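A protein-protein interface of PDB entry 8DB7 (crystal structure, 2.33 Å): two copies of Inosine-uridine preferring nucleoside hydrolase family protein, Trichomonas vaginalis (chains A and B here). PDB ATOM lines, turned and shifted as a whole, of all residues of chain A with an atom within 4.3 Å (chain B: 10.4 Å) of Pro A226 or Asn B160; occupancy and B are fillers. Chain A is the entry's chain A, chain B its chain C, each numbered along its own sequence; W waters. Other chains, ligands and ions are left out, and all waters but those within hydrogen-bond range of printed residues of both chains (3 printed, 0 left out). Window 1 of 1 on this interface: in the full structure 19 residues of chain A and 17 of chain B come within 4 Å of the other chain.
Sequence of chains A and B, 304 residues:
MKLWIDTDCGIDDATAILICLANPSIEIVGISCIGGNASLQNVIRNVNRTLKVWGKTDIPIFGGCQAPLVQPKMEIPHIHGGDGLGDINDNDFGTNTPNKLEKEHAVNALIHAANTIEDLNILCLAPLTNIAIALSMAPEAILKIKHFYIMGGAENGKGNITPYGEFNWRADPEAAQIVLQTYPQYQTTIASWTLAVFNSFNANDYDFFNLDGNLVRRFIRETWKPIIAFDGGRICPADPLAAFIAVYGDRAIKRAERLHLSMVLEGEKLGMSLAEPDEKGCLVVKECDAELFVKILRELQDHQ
Of the 21 printed residues of chain B, 6 touch a printed residue of chain A. Of the 11 printed residues of chain A, 5 touch a printed residue of chain B. Among the printed residues, 9 pairs touch across the chains.
NE of Arg B234 lies close to O of Phe A230, 3.5 Å away.
No position is printed for both chains. Of the 9 pairs that touch across the chains among the printed residues, none has its exchanged pair printed and touching as well.
Of the printed residues of chain B, Ile A79 touches Asp B231 (3.8 Å). No residue of chain B comes within 4 Å of Gly A86. Of the printed residues of chain B, Lys A225 touches Asn B160 (3.3 Å). Of chain B, only Asn B160 (3.2 Å) and Thr B162 (3.6 Å) come within 4 Å of Pro A226. No residue of chain B comes within 4 Å of Ile A227. Ile A228 touches none of the printed residues of chain B. Ala A229 touches just these residues of chain B: Asn B160 (3.6 Å) and Ile B161 (3.7 Å). Printed residues of chain B within 4 Å of Phe A230: Val B197 (3.8 Å), Asp B231 (3.5 Å) and Arg B234 (3.1 Å). Of chain A, only Lys A225, Pro A226 and Ala A229 come within 4 Å of Asn B160. Of the printed residues of chain A, Thr B162 touches Pro A226. Thr B194 touches none of the printed residues of chain A. Printed residues of chain A within 4 Å of Asp B231: Ile A79 (3.8 Å) and Phe A230 (3.5 Å). Of the printed residues of chain A, Arg B234 touches Phe A230 (3.1 Å). The nearest printed residue of chain A that does not touch Asn B160 is Ile A227 (5.4 Å). The nearest printed residue of chain A that does not touch Asp B231 is Ile A227 (9.1 Å).
The side-chain amino group of Lys A225 is in salt-bridge range of the side-chain carboxylate of Glu A222 (2.9 Å). O of Val B197 is in hydrogen-bond range of OG of Ser B200. The side-chain hydroxyl (OG) of Ser B200 is in hydrogen-bond range of the guanidinium group (NH2) of Arg B234 (2.8 Å).
Water W3 bridges O of Lys A225 (2.7 Å) and ND2 of Asn B160 (2.8 Å). Water W1 lies within hydrogen-bond range of the backbone carbonyl oxygen (O) of Val B197 (2.7 Å) and the backbone carbonyl oxygen (O) of Ala A229 (2.9 Å). Water W2 bridges N of Thr B162 (3.0 Å) and O of Pro A226 (3.1 Å).
Among the printed residues, pairs that only touch across the chains: Ile A79 with Asp B231 (3.8 Å), Lys A225 with Asn B160 (3.3 Å), Pro A226 with Asn B160 (3.2 Å), Pro A226 with Thr B162 (3.6 Å), Ala A229 with Asn B160 (3.6 Å), Ala A229 with Ile B161 (3.7 Å), Phe A230 with Val B197 (3.8 Å) and Phe A230 with Asp B231 (3.5 Å).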
ATOM      1  N   ILE A  79      -9.604  18.161 -30.200  1.00  0.00           N
ATOM      2  CA  ILE A  79      -8.264  18.554 -30.608  1.00  0.00           C
ATOM      3  C   ILE A  79      -8.253  19.107 -32.024  1.00  0.00           C
ATOM      4  O   ILE A  79      -7.579  20.112 -32.303  1.00  0.00           O
ATOM      5  CB  ILE A  79      -7.270  17.366 -30.483  1.00  0.00           C
ATOM      6  CG1 ILE A  79      -7.189  16.885 -29.028  1.00  0.00           C
ATOM      7  CG2 ILE A  79      -5.875  17.753 -31.015  1.00  0.00           C
ATOM      8  CD1 ILE A  79      -6.263  15.693 -28.809  1.00  0.00           C
ATOM      9  N   GLY A  86     -10.835  21.833 -37.636  1.00  0.00           N
ATOM     10  CA  GLY A  86     -10.935  23.053 -36.866  1.00  0.00           C
ATOM     11  C   GLY A  86     -12.202  23.843 -37.077  1.00  0.00           C
ATOM     12  O   GLY A  86     -12.229  25.033 -36.761  1.00  0.00           O
ATOM     13  N   GLU A 222      -6.550  29.625 -39.408  1.00  0.00           N
ATOM     14  CA  GLU A 222      -7.821  29.187 -38.835  1.00  0.00           C
ATOM     15  C   GLU A 222      -7.797  27.703 -38.482  1.00  0.00           C
ATOM     16  O   GLU A 222      -8.301  27.307 -37.426  1.00  0.00           O
ATOM     17  CB  GLU A 222      -8.974  29.475 -39.800  1.00  0.00           C
ATOM     18  CG  GLU A 222      -9.248  30.953 -40.067  1.00  0.00           C
ATOM     19  CD  GLU A 222      -9.323  31.782 -38.799  1.00  0.00           C
ATOM     20  OE1 GLU A 222     -10.181  31.498 -37.934  1.00  0.00           O
ATOM     21  OE2 GLU A 222      -8.510  32.725 -38.664  1.00  0.00           O
ATOM     22  N   THR A 223      -7.223  26.866 -39.348  1.00  0.00           N
ATOM     23  CA  THR A 223      -7.231  25.437 -39.054  1.00  0.00           C
ATOM     24  C   THR A 223      -6.332  25.085 -37.874  1.00  0.00           C
ATOM     25  O   THR A 223      -6.672  24.177 -37.118  1.00  0.00           O
ATOM     26  CB  THR A 223      -6.842  24.621 -40.283  1.00  0.00           C
ATOM     27  OG1 THR A 223      -5.549  25.025 -40.736  1.00  0.00           O
ATOM     28  CG2 THR A 223      -7.899  24.811 -41.419  1.00  0.00           C
ATOM     29  N   TRP A 224      -5.240  25.823 -37.646  1.00  0.00           N
ATOM     30  CA  TRP A 224      -4.328  25.483 -36.547  1.00  0.00           C
ATOM     31  C   TRP A 224      -4.744  26.064 -35.204  1.00  0.00           C
ATOM     32  O   TRP A 224      -4.213  25.638 -34.179  1.00  0.00           O
ATOM     33  CB  TRP A 224      -2.894  25.920 -36.862  1.00  0.00           C
ATOM     34  CG  TRP A 224      -2.143  24.906 -37.686  1.00  0.00           C
ATOM     35  CD1 TRP A 224      -2.104  24.823 -39.049  1.00  0.00           C
ATOM     36  CD2 TRP A 224      -1.358  23.811 -37.195  1.00  0.00           C
ATOM     37  NE1 TRP A 224      -1.324  23.758 -39.435  1.00  0.00           N
ATOM     38  CE2 TRP A 224      -0.866  23.114 -38.313  1.00  0.00           C
ATOM     39  CE3 TRP A 224      -1.024  23.358 -35.921  1.00  0.00           C
ATOM     40  CZ2 TRP A 224      -0.048  21.991 -38.191  1.00  0.00           C
ATOM     41  CZ3 TRP A 224      -0.206  22.259 -35.799  1.00  0.00           C
ATOM     42  CH2 TRP A 224       0.271  21.580 -36.930  1.00  0.00           C
ATOM     43  N   LYS A 225      -5.683  26.999 -35.175  1.00  0.00           N
ATOM     44  CA  LYS A 225      -6.162  27.592 -33.929  1.00  0.00           C
ATOM     45  C   LYS A 225      -6.495  26.552 -32.847  1.00  0.00           C
ATOM     46  O   LYS A 225      -5.913  26.604 -31.748  1.00  0.00           O
ATOM     47  CB  LYS A 225      -7.381  28.476 -34.229  1.00  0.00           C
ATOM     48  CG  LYS A 225      -7.043  29.878 -34.740  1.00  0.00           C
ATOM     49  CD  LYS A 225      -8.266  30.788 -34.653  1.00  0.00           C
ATOM     50  CE  LYS A 225      -8.079  32.077 -35.431  1.00  0.00           C
ATOM     51  NZ  LYS A 225      -9.373  32.831 -35.536  1.00  0.00           N
ATOM     52  N   PRO A 226      -7.403  25.593 -33.105  1.00  0.00           N
ATOM     53  CA  PRO A 226      -7.842  24.699 -32.012  1.00  0.00           C
ATOM     54  C   PRO A 226      -6.741  23.804 -31.475  1.00  0.00           C
ATOM     55  O   PRO A 226      -6.662  23.567 -30.259  1.00  0.00           O
ATOM     56  CB  PRO A 226      -8.953  23.852 -32.663  1.00  0.00           C
ATOM     57  CG  PRO A 226      -9.138  24.389 -34.029  1.00  0.00           C
ATOM     58  CD  PRO A 226      -7.947  25.168 -34.406  1.00  0.00           C
ATOM     59  N   ILE A 227      -5.899  23.272 -32.365  1.00  0.00           N
ATOM     60  CA  ILE A 227      -4.891  22.329 -31.921  1.00  0.00           C
ATOM     61  C   ILE A 227      -3.786  23.064 -31.165  1.00  0.00           C
ATOM     62  O   ILE A 227      -3.312  22.590 -30.121  1.00  0.00           O
ATOM     63  CB  ILE A 227      -4.387  21.490 -33.121  1.00  0.00           C
ATOM     64  CG1 ILE A 227      -3.370  20.420 -32.695  1.00  0.00           C
ATOM     65  CG2 ILE A 227      -3.866  22.361 -34.258  1.00  0.00           C
ATOM     66  CD1 ILE A 227      -3.237  19.271 -33.707  1.00  0.00           C
ATOM     67  N   ILE A 228      -3.410  24.264 -31.625  1.00  0.00           N
ATOM     68  CA  ILE A 228      -2.440  25.065 -30.875  1.00  0.00           C
ATOM     69  C   ILE A 228      -2.965  25.362 -29.482  1.00  0.00           C
ATOM     70  O   ILE A 228      -2.255  25.182 -28.487  1.00  0.00           O
ATOM     71  CB  ILE A 228      -2.102  26.361 -31.627  1.00  0.00           C
ATOM     72  CG1 ILE A 228      -1.207  26.059 -32.827  1.00  0.00           C
ATOM     73  CG2 ILE A 228      -1.466  27.384 -30.678  1.00  0.00           C
ATOM     74  CD1 ILE A 228      -1.204  27.151 -33.856  1.00  0.00           C
ATOM     75  N   ALA A 229      -4.212  25.842 -29.385  1.00  0.00           N
ATOM     76  CA  ALA A 229      -4.781  26.117 -28.066  1.00  0.00           C
ATOM     77  C   ALA A 229      -4.853  24.850 -27.215  1.00  0.00           C
ATOM     78  O   ALA A 229      -4.640  24.895 -25.997  1.00  0.00           O
ATOM     79  CB  ALA A 229      -6.168  26.739 -28.198  1.00  0.00           C
ATOM     80  N   PHE A 230      -5.161  23.728 -27.856  1.00  0.00           N
ATOM     81  CA  PHE A 230      -5.267  22.452 -27.158  1.00  0.00           C
ATOM     82  C   PHE A 230      -3.899  21.902 -26.771  1.00  0.00           C
ATOM     83  O   PHE A 230      -3.797  20.971 -25.971  1.00  0.00           O
ATOM     84  CB  PHE A 230      -6.016  21.432 -28.019  1.00  0.00           C
ATOM     85  CG  PHE A 230      -5.989  20.035 -27.465  1.00  0.00           C
ATOM     86  CD1 PHE A 230      -7.048  19.554 -26.713  1.00  0.00           C
ATOM     87  CD2 PHE A 230      -4.905  19.205 -27.696  1.00  0.00           C
ATOM     88  CE1 PHE A 230      -7.026  18.269 -26.202  1.00  0.00           C
ATOM     89  CE2 PHE A 230      -4.876  17.921 -27.188  1.00  0.00           C
ATOM     90  CZ  PHE A 230      -5.939  17.451 -26.440  1.00  0.00           C
ATOM     91  N   ALA B 154     -18.838  24.543 -22.325  1.00  0.00           N
ATOM     92  CA  ALA B 154     -17.629  25.009 -22.983  1.00  0.00           C
ATOM     93  C   ALA B 154     -17.893  26.397 -23.537  1.00  0.00           C
ATOM     94  O   ALA B 154     -19.013  26.721 -23.930  1.00  0.00           O
ATOM     95  CB  ALA B 154     -17.189  24.079 -24.114  1.00  0.00           C
ATOM     96  N   GLU B 155     -16.864  27.192 -23.678  1.00  0.00           N
ATOM     97  CA  GLU B 155     -17.030  28.475 -24.270  1.00  0.00           C
ATOM     98  C   GLU B 155     -17.034  28.288 -25.765  1.00  0.00           C
ATOM     99  O   GLU B 155     -16.332  27.490 -26.320  1.00  0.00           O
ATOM    100  CB  GLU B 155     -16.005  29.481 -23.803  1.00  0.00           C
ATOM    101  CG  GLU B 155     -16.141  29.848 -22.319  1.00  0.00           C
ATOM    102  CD  GLU B 155     -17.480  30.459 -21.861  1.00  0.00           C
ATOM    103  OE1 GLU B 155     -17.657  31.670 -22.041  1.00  0.00           O
ATOM    104  OE2 GLU B 155     -18.316  29.755 -21.252  1.00  0.00           O
ATOM    105  N   ASN B 156     -17.915  28.999 -26.410  1.00  0.00           N
ATOM    106  CA  ASN B 156     -18.060  28.852 -27.809  1.00  0.00           C
ATOM    107  C   ASN B 156     -18.021  30.233 -28.310  1.00  0.00           C
ATOM    108  O   ASN B 156     -18.983  30.976 -28.337  1.00  0.00           O
ATOM    109  CB  ASN B 156     -19.377  28.208 -28.162  1.00  0.00           C
ATOM    110  CG  ASN B 156     -19.809  28.553 -29.554  1.00  0.00           C
ATOM    111  OD1 ASN B 156     -19.046  28.421 -30.489  1.00  0.00           O
ATOM    112  ND2 ASN B 156     -21.036  29.007 -29.694  1.00  0.00           N
ATOM    113  N   GLY B 157     -16.820  30.585 -28.690  1.00  0.00           N
ATOM    114  CA  GLY B 157     -16.546  31.921 -29.135  1.00  0.00           C
ATOM    115  C   GLY B 157     -15.795  32.544 -27.997  1.00  0.00           C
ATOM    116  O   GLY B 157     -16.012  32.205 -26.806  1.00  0.00           O
ATOM    117  N   LYS B 158     -14.917  33.441 -28.424  1.00  0.00           N
ATOM    118  CA  LYS B 158     -13.977  34.249 -27.642  1.00  0.00           C
ATOM    119  C   LYS B 158     -12.887  33.351 -27.061  1.00  0.00           C
ATOM    120  O   LYS B 158     -12.622  33.362 -25.859  1.00  0.00           O
ATOM    121  CB  LYS B 158     -14.689  35.044 -26.541  1.00  0.00           C
ATOM    122  CG  LYS B 158     -15.048  36.466 -26.939  1.00  0.00           C
ATOM    123  CD  LYS B 158     -14.231  36.928 -28.134  1.00  0.00           C
ATOM    124  CE  LYS B 158     -15.096  37.051 -29.379  1.00  0.00           C
ATOM    125  NZ  LYS B 158     -14.676  38.195 -30.235  1.00  0.00           N
ATOM    126  N   GLY B 159     -12.265  32.573 -27.940  1.00  0.00           N
ATOM    127  CA  GLY B 159     -11.230  31.633 -27.569  1.00  0.00           C
ATOM    128  C   GLY B 159     -10.912  30.747 -28.756  1.00  0.00           C
ATOM    129  O   GLY B 159     -11.527  30.867 -29.815  1.00  0.00           O
ATOM    130  N   ASN B 160      -9.964  29.838 -28.566  1.00  0.00           N
ATOM    131  CA  ASN B 160      -9.513  28.943 -29.616  1.00  0.00           C
ATOM    132  C   ASN B 160      -9.692  27.464 -29.277  1.00  0.00           C
ATOM    133  O   ASN B 160      -9.543  26.620 -30.171  1.00  0.00           O
ATOM    134  CB  ASN B 160      -8.053  29.257 -29.966  1.00  0.00           C
ATOM    135  CG  ASN B 160      -7.934  30.458 -30.906  1.00  0.00           C
ATOM    136  OD1 ASN B 160      -8.944  30.968 -31.407  1.00  0.00           O
ATOM    137  ND2 ASN B 160      -6.694  30.918 -31.147  1.00  0.00           N
ATOM    138  N   ILE B 161     -10.044  27.142 -28.033  1.00  0.00           N
ATOM    139  CA  ILE B 161     -10.303  25.774 -27.583  1.00  0.00           C
ATOM    140  C   ILE B 161     -11.695  25.343 -28.054  1.00  0.00           C
ATOM    141  O   ILE B 161     -12.700  25.956 -27.674  1.00  0.00           O
ATOM    142  CB  ILE B 161     -10.182  25.681 -26.053  1.00  0.00           C
ATOM    143  CG1 ILE B 161      -8.744  26.020 -25.619  1.00  0.00           C
ATOM    144  CG2 ILE B 161     -10.670  24.301 -25.510  1.00  0.00           C
ATOM    145  CD1 ILE B 161      -8.626  26.464 -24.160  1.00  0.00           C
ATOM    146  N   THR B 162     -11.745  24.273 -28.863  1.00  0.00           N
ATOM    147  CA  THR B 162     -12.997  23.800 -29.459  1.00  0.00           C
ATOM    148  C   THR B 162     -14.065  23.617 -28.405  1.00  0.00           C
ATOM    149  O   THR B 162     -13.821  22.950 -27.385  1.00  0.00           O
ATOM    150  CB  THR B 162     -12.859  22.439 -30.156  1.00  0.00           C
ATOM    151  OG1 THR B 162     -11.582  22.281 -30.795  1.00  0.00           O
ATOM    152  CG2 THR B 162     -13.974  22.282 -31.158  1.00  0.00           C
ATOM    153  N   PRO B 163     -15.282  24.124 -28.602  1.00  0.00           N
ATOM    154  CA  PRO B 163     -16.404  23.687 -27.785  1.00  0.00           C
ATOM    155  C   PRO B 163     -16.739  22.216 -27.996  1.00  0.00           C
ATOM    156  O   PRO B 163     -17.441  21.629 -27.162  1.00  0.00           O
ATOM    157  CB  PRO B 163     -17.546  24.600 -28.245  1.00  0.00           C
ATOM    158  CG  PRO B 163     -17.182  24.923 -29.665  1.00  0.00           C
ATOM    159  CD  PRO B 163     -15.694  25.133 -29.601  1.00  0.00           C
ATOM    160  N   TYR B 164     -16.245  21.597 -29.075  1.00  0.00           N
ATOM    161  CA  TYR B 164     -16.601  20.216 -29.393  1.00  0.00           C
ATOM    162  C   TYR B 164     -15.883  19.186 -28.525  1.00  0.00           C
ATOM    163  O   TYR B 164     -16.062  17.979 -28.745  1.00  0.00           O
ATOM    164  CB  TYR B 164     -16.333  19.928 -30.867  1.00  0.00           C
ATOM    165  CG  TYR B 164     -17.334  20.596 -31.774  1.00  0.00           C
ATOM    166  CD1 TYR B 164     -18.532  19.988 -32.076  1.00  0.00           C
ATOM    167  CD2 TYR B 164     -17.084  21.855 -32.311  1.00  0.00           C
ATOM    168  CE1 TYR B 164     -19.440  20.598 -32.894  1.00  0.00           C
ATOM    169  CE2 TYR B 164     -17.993  22.473 -33.122  1.00  0.00           C
ATOM    170  CZ  TYR B 164     -19.166  21.836 -33.416  1.00  0.00           C
ATOM    171  OH  TYR B 164     -20.076  22.447 -34.230  1.00  0.00           O
ATOM    172  N   GLY B 165     -15.058  19.617 -27.571  1.00  0.00           N
ATOM    173  CA  GLY B 165     -14.616  18.642 -26.591  1.00  0.00           C
ATOM    174  C   GLY B 165     -15.601  18.374 -25.481  1.00  0.00           C
ATOM    175  O   GLY B 165     -15.416  17.420 -24.726  1.00  0.00           O
ATOM    176  N   TRP B 193     -15.393  22.529 -19.709  1.00  0.00           N
ATOM    177  CA  TRP B 193     -14.448  21.791 -20.533  1.00  0.00           C
ATOM    178  C   TRP B 193     -13.370  22.708 -21.081  1.00  0.00           C
ATOM    179  O   TRP B 193     -12.226  22.280 -21.255  1.00  0.00           O
ATOM    180  CB  TRP B 193     -15.161  21.070 -21.681  1.00  0.00           C
ATOM    181  CG  TRP B 193     -14.188  20.592 -22.682  1.00  0.00           C
ATOM    182  CD1 TRP B 193     -13.962  21.109 -23.916  1.00  0.00           C
ATOM    183  CD2 TRP B 193     -13.234  19.533 -22.500  1.00  0.00           C
ATOM    184  NE1 TRP B 193     -12.940  20.421 -24.535  1.00  0.00           N
ATOM    185  CE2 TRP B 193     -12.481  19.442 -23.687  1.00  0.00           C
ATOM    186  CE3 TRP B 193     -12.958  18.640 -21.453  1.00  0.00           C
ATOM    187  CZ2 TRP B 193     -11.458  18.493 -23.857  1.00  0.00           C
ATOM    188  CZ3 TRP B 193     -11.944  17.683 -21.633  1.00  0.00           C
ATOM    189  CH2 TRP B 193     -11.203  17.633 -22.821  1.00  0.00           C
ATOM    190  N   THR B 194     -13.718  23.964 -21.371  1.00  0.00           N
ATOM    191  CA  THR B 194     -12.697  24.953 -21.706  1.00  0.00           C
ATOM    192  C   THR B 194     -11.635  25.022 -20.609  1.00  0.00           C
ATOM    193  O   THR B 194     -10.434  24.959 -20.891  1.00  0.00           O
ATOM    194  CB  THR B 194     -13.357  26.320 -21.919  1.00  0.00           C
ATOM    195  OG1 THR B 194     -14.442  26.172 -22.832  1.00  0.00           O
ATOM    196  CG2 THR B 194     -12.350  27.349 -22.475  1.00  0.00           C
ATOM    197  N   VAL B 197      -9.075  22.203 -20.652  1.00  0.00           N
ATOM    198  CA  VAL B 197      -8.019  22.280 -21.669  1.00  0.00           C
ATOM    199  C   VAL B 197      -7.055  23.418 -21.351  1.00  0.00           C
ATOM    200  O   VAL B 197      -5.840  23.303 -21.549  1.00  0.00           O
ATOM    201  CB  VAL B 197      -8.624  22.442 -23.083  1.00  0.00           C
ATOM    202  CG1 VAL B 197      -7.516  22.664 -24.137  1.00  0.00           C
ATOM    203  CG2 VAL B 197      -9.482  21.242 -23.448  1.00  0.00           C
ATOM    204  N   PHE B 198      -7.582  24.538 -20.863  1.00  0.00           N
ATOM    205  CA  PHE B 198      -6.717  25.652 -20.499  1.00  0.00           C
ATOM    206  C   PHE B 198      -5.812  25.279 -19.330  1.00  0.00           C
ATOM    207  O   PHE B 198      -4.595  25.489 -19.382  1.00  0.00           O
ATOM    208  CB  PHE B 198      -7.558  26.888 -20.187  1.00  0.00           C
ATOM    209  CG  PHE B 198      -6.753  28.050 -19.739  1.00  0.00           C
ATOM    210  CD1 PHE B 198      -6.191  28.912 -20.665  1.00  0.00           C
ATOM    211  CD2 PHE B 198      -6.539  28.278 -18.389  1.00  0.00           C
ATOM    212  CE1 PHE B 198      -5.424  29.989 -20.248  1.00  0.00           C
ATOM    213  CE2 PHE B 198      -5.772  29.350 -17.972  1.00  0.00           C
ATOM    214  CZ  PHE B 198      -5.219  30.210 -18.896  1.00  0.00           C
ATOM    215  N   SER B 200      -4.812  22.340 -18.545  1.00  0.00           N
ATOM    216  CA  SER B 200      -4.322  20.993 -18.774  1.00  0.00           C
ATOM    217  C   SER B 200      -2.801  20.939 -18.594  1.00  0.00           C
ATOM    218  O   SER B 200      -2.118  21.963 -18.499  1.00  0.00           O
ATOM    219  CB  SER B 200      -4.719  20.516 -20.169  1.00  0.00           C
ATOM    220  OG  SER B 200      -3.814  21.036 -21.121  1.00  0.00           O
ATOM    221  N   ASP B 231      -6.291  12.461 -26.137  1.00  0.00           N
ATOM    222  CA  ASP B 231      -5.822  13.758 -25.615  1.00  0.00           C
ATOM    223  C   ASP B 231      -4.332  14.001 -25.859  1.00  0.00           C
ATOM    224  O   ASP B 231      -3.776  14.937 -25.299  1.00  0.00           O
ATOM    225  CB  ASP B 231      -6.093  13.954 -24.110  1.00  0.00           C
ATOM    226  CG  ASP B 231      -7.564  13.728 -23.722  1.00  0.00           C
ATOM    227  OD1 ASP B 231      -8.404  13.456 -24.599  1.00  0.00           O
ATOM    228  OD2 ASP B 231      -7.892  13.848 -22.521  1.00  0.00           O
ATOM    229  N   ARG B 234      -1.594  14.603 -23.130  1.00  0.00           N
ATOM    230  CA  ARG B 234      -1.973  15.645 -22.189  1.00  0.00           C
ATOM    231  C   ARG B 234      -2.930  15.133 -21.115  1.00  0.00           C
ATOM    232  O   ARG B 234      -3.761  14.246 -21.349  1.00  0.00           O
ATOM    233  CB  ARG B 234      -2.624  16.821 -22.930  1.00  0.00           C
ATOM    234  CG  ARG B 234      -1.671  17.612 -23.812  1.00  0.00           C
ATOM    235  CD  ARG B 234      -2.254  18.951 -24.170  1.00  0.00           C
ATOM    236  NE  ARG B 234      -2.163  19.913 -23.064  1.00  0.00           N
ATOM    237  CZ  ARG B 234      -1.091  20.650 -22.771  1.00  0.00           C
ATOM    238  NH1 ARG B 234       0.031  20.544 -23.489  1.00  0.00           N
ATOM    239  NH2 ARG B 234      -1.146  21.493 -21.743  1.00  0.00           N
ATOM    240  N   CYS B 236      -5.998  16.415 -19.215  1.00  0.00           N
ATOM    241  CA  CYS B 236      -7.069  17.407 -19.206  1.00  0.00           C
ATOM    242  C   CYS B 236      -7.990  17.108 -18.033  1.00  0.00           C
ATOM    243  O   CYS B 236      -8.969  16.366 -18.182  1.00  0.00           O
ATOM    244  CB  CYS B 236      -7.830  17.375 -20.534  1.00  0.00           C
ATOM    245  SG  CYS B 236      -6.773  17.495 -22.018  1.00  0.00           S
ATOM    246  N   LYS B 286     -12.476  30.532 -14.922  1.00  0.00           N
ATOM    247  CA  LYS B 286     -11.665  30.664 -16.122  1.00  0.00           C
ATOM    248  C   LYS B 286     -10.250  30.150 -15.940  1.00  0.00           C
ATOM    249  O   LYS B 286      -9.626  29.709 -16.917  1.00  0.00           O
ATOM    250  CB  LYS B 286     -11.625  32.133 -16.561  1.00  0.00           C
ATOM    251  CG  LYS B 286     -12.996  32.725 -16.869  1.00  0.00           C
ATOM    252  CD  LYS B 286     -13.568  32.105 -18.136  1.00  0.00           C
ATOM    253  CE  LYS B 286     -14.828  32.806 -18.597  1.00  0.00           C
ATOM    254  NZ  LYS B 286     -14.916  32.832 -20.080  1.00  0.00           N
HETATM  255  O   HOH W   1      -3.921  23.776 -23.415  1.00  0.00           O
HETATM  256  O   HOH W   2      -9.211  22.765 -28.771  1.00  0.00           O
HETATM  257  O   HOH W   3      -4.741  28.895 -31.013  1.00  0.00           O
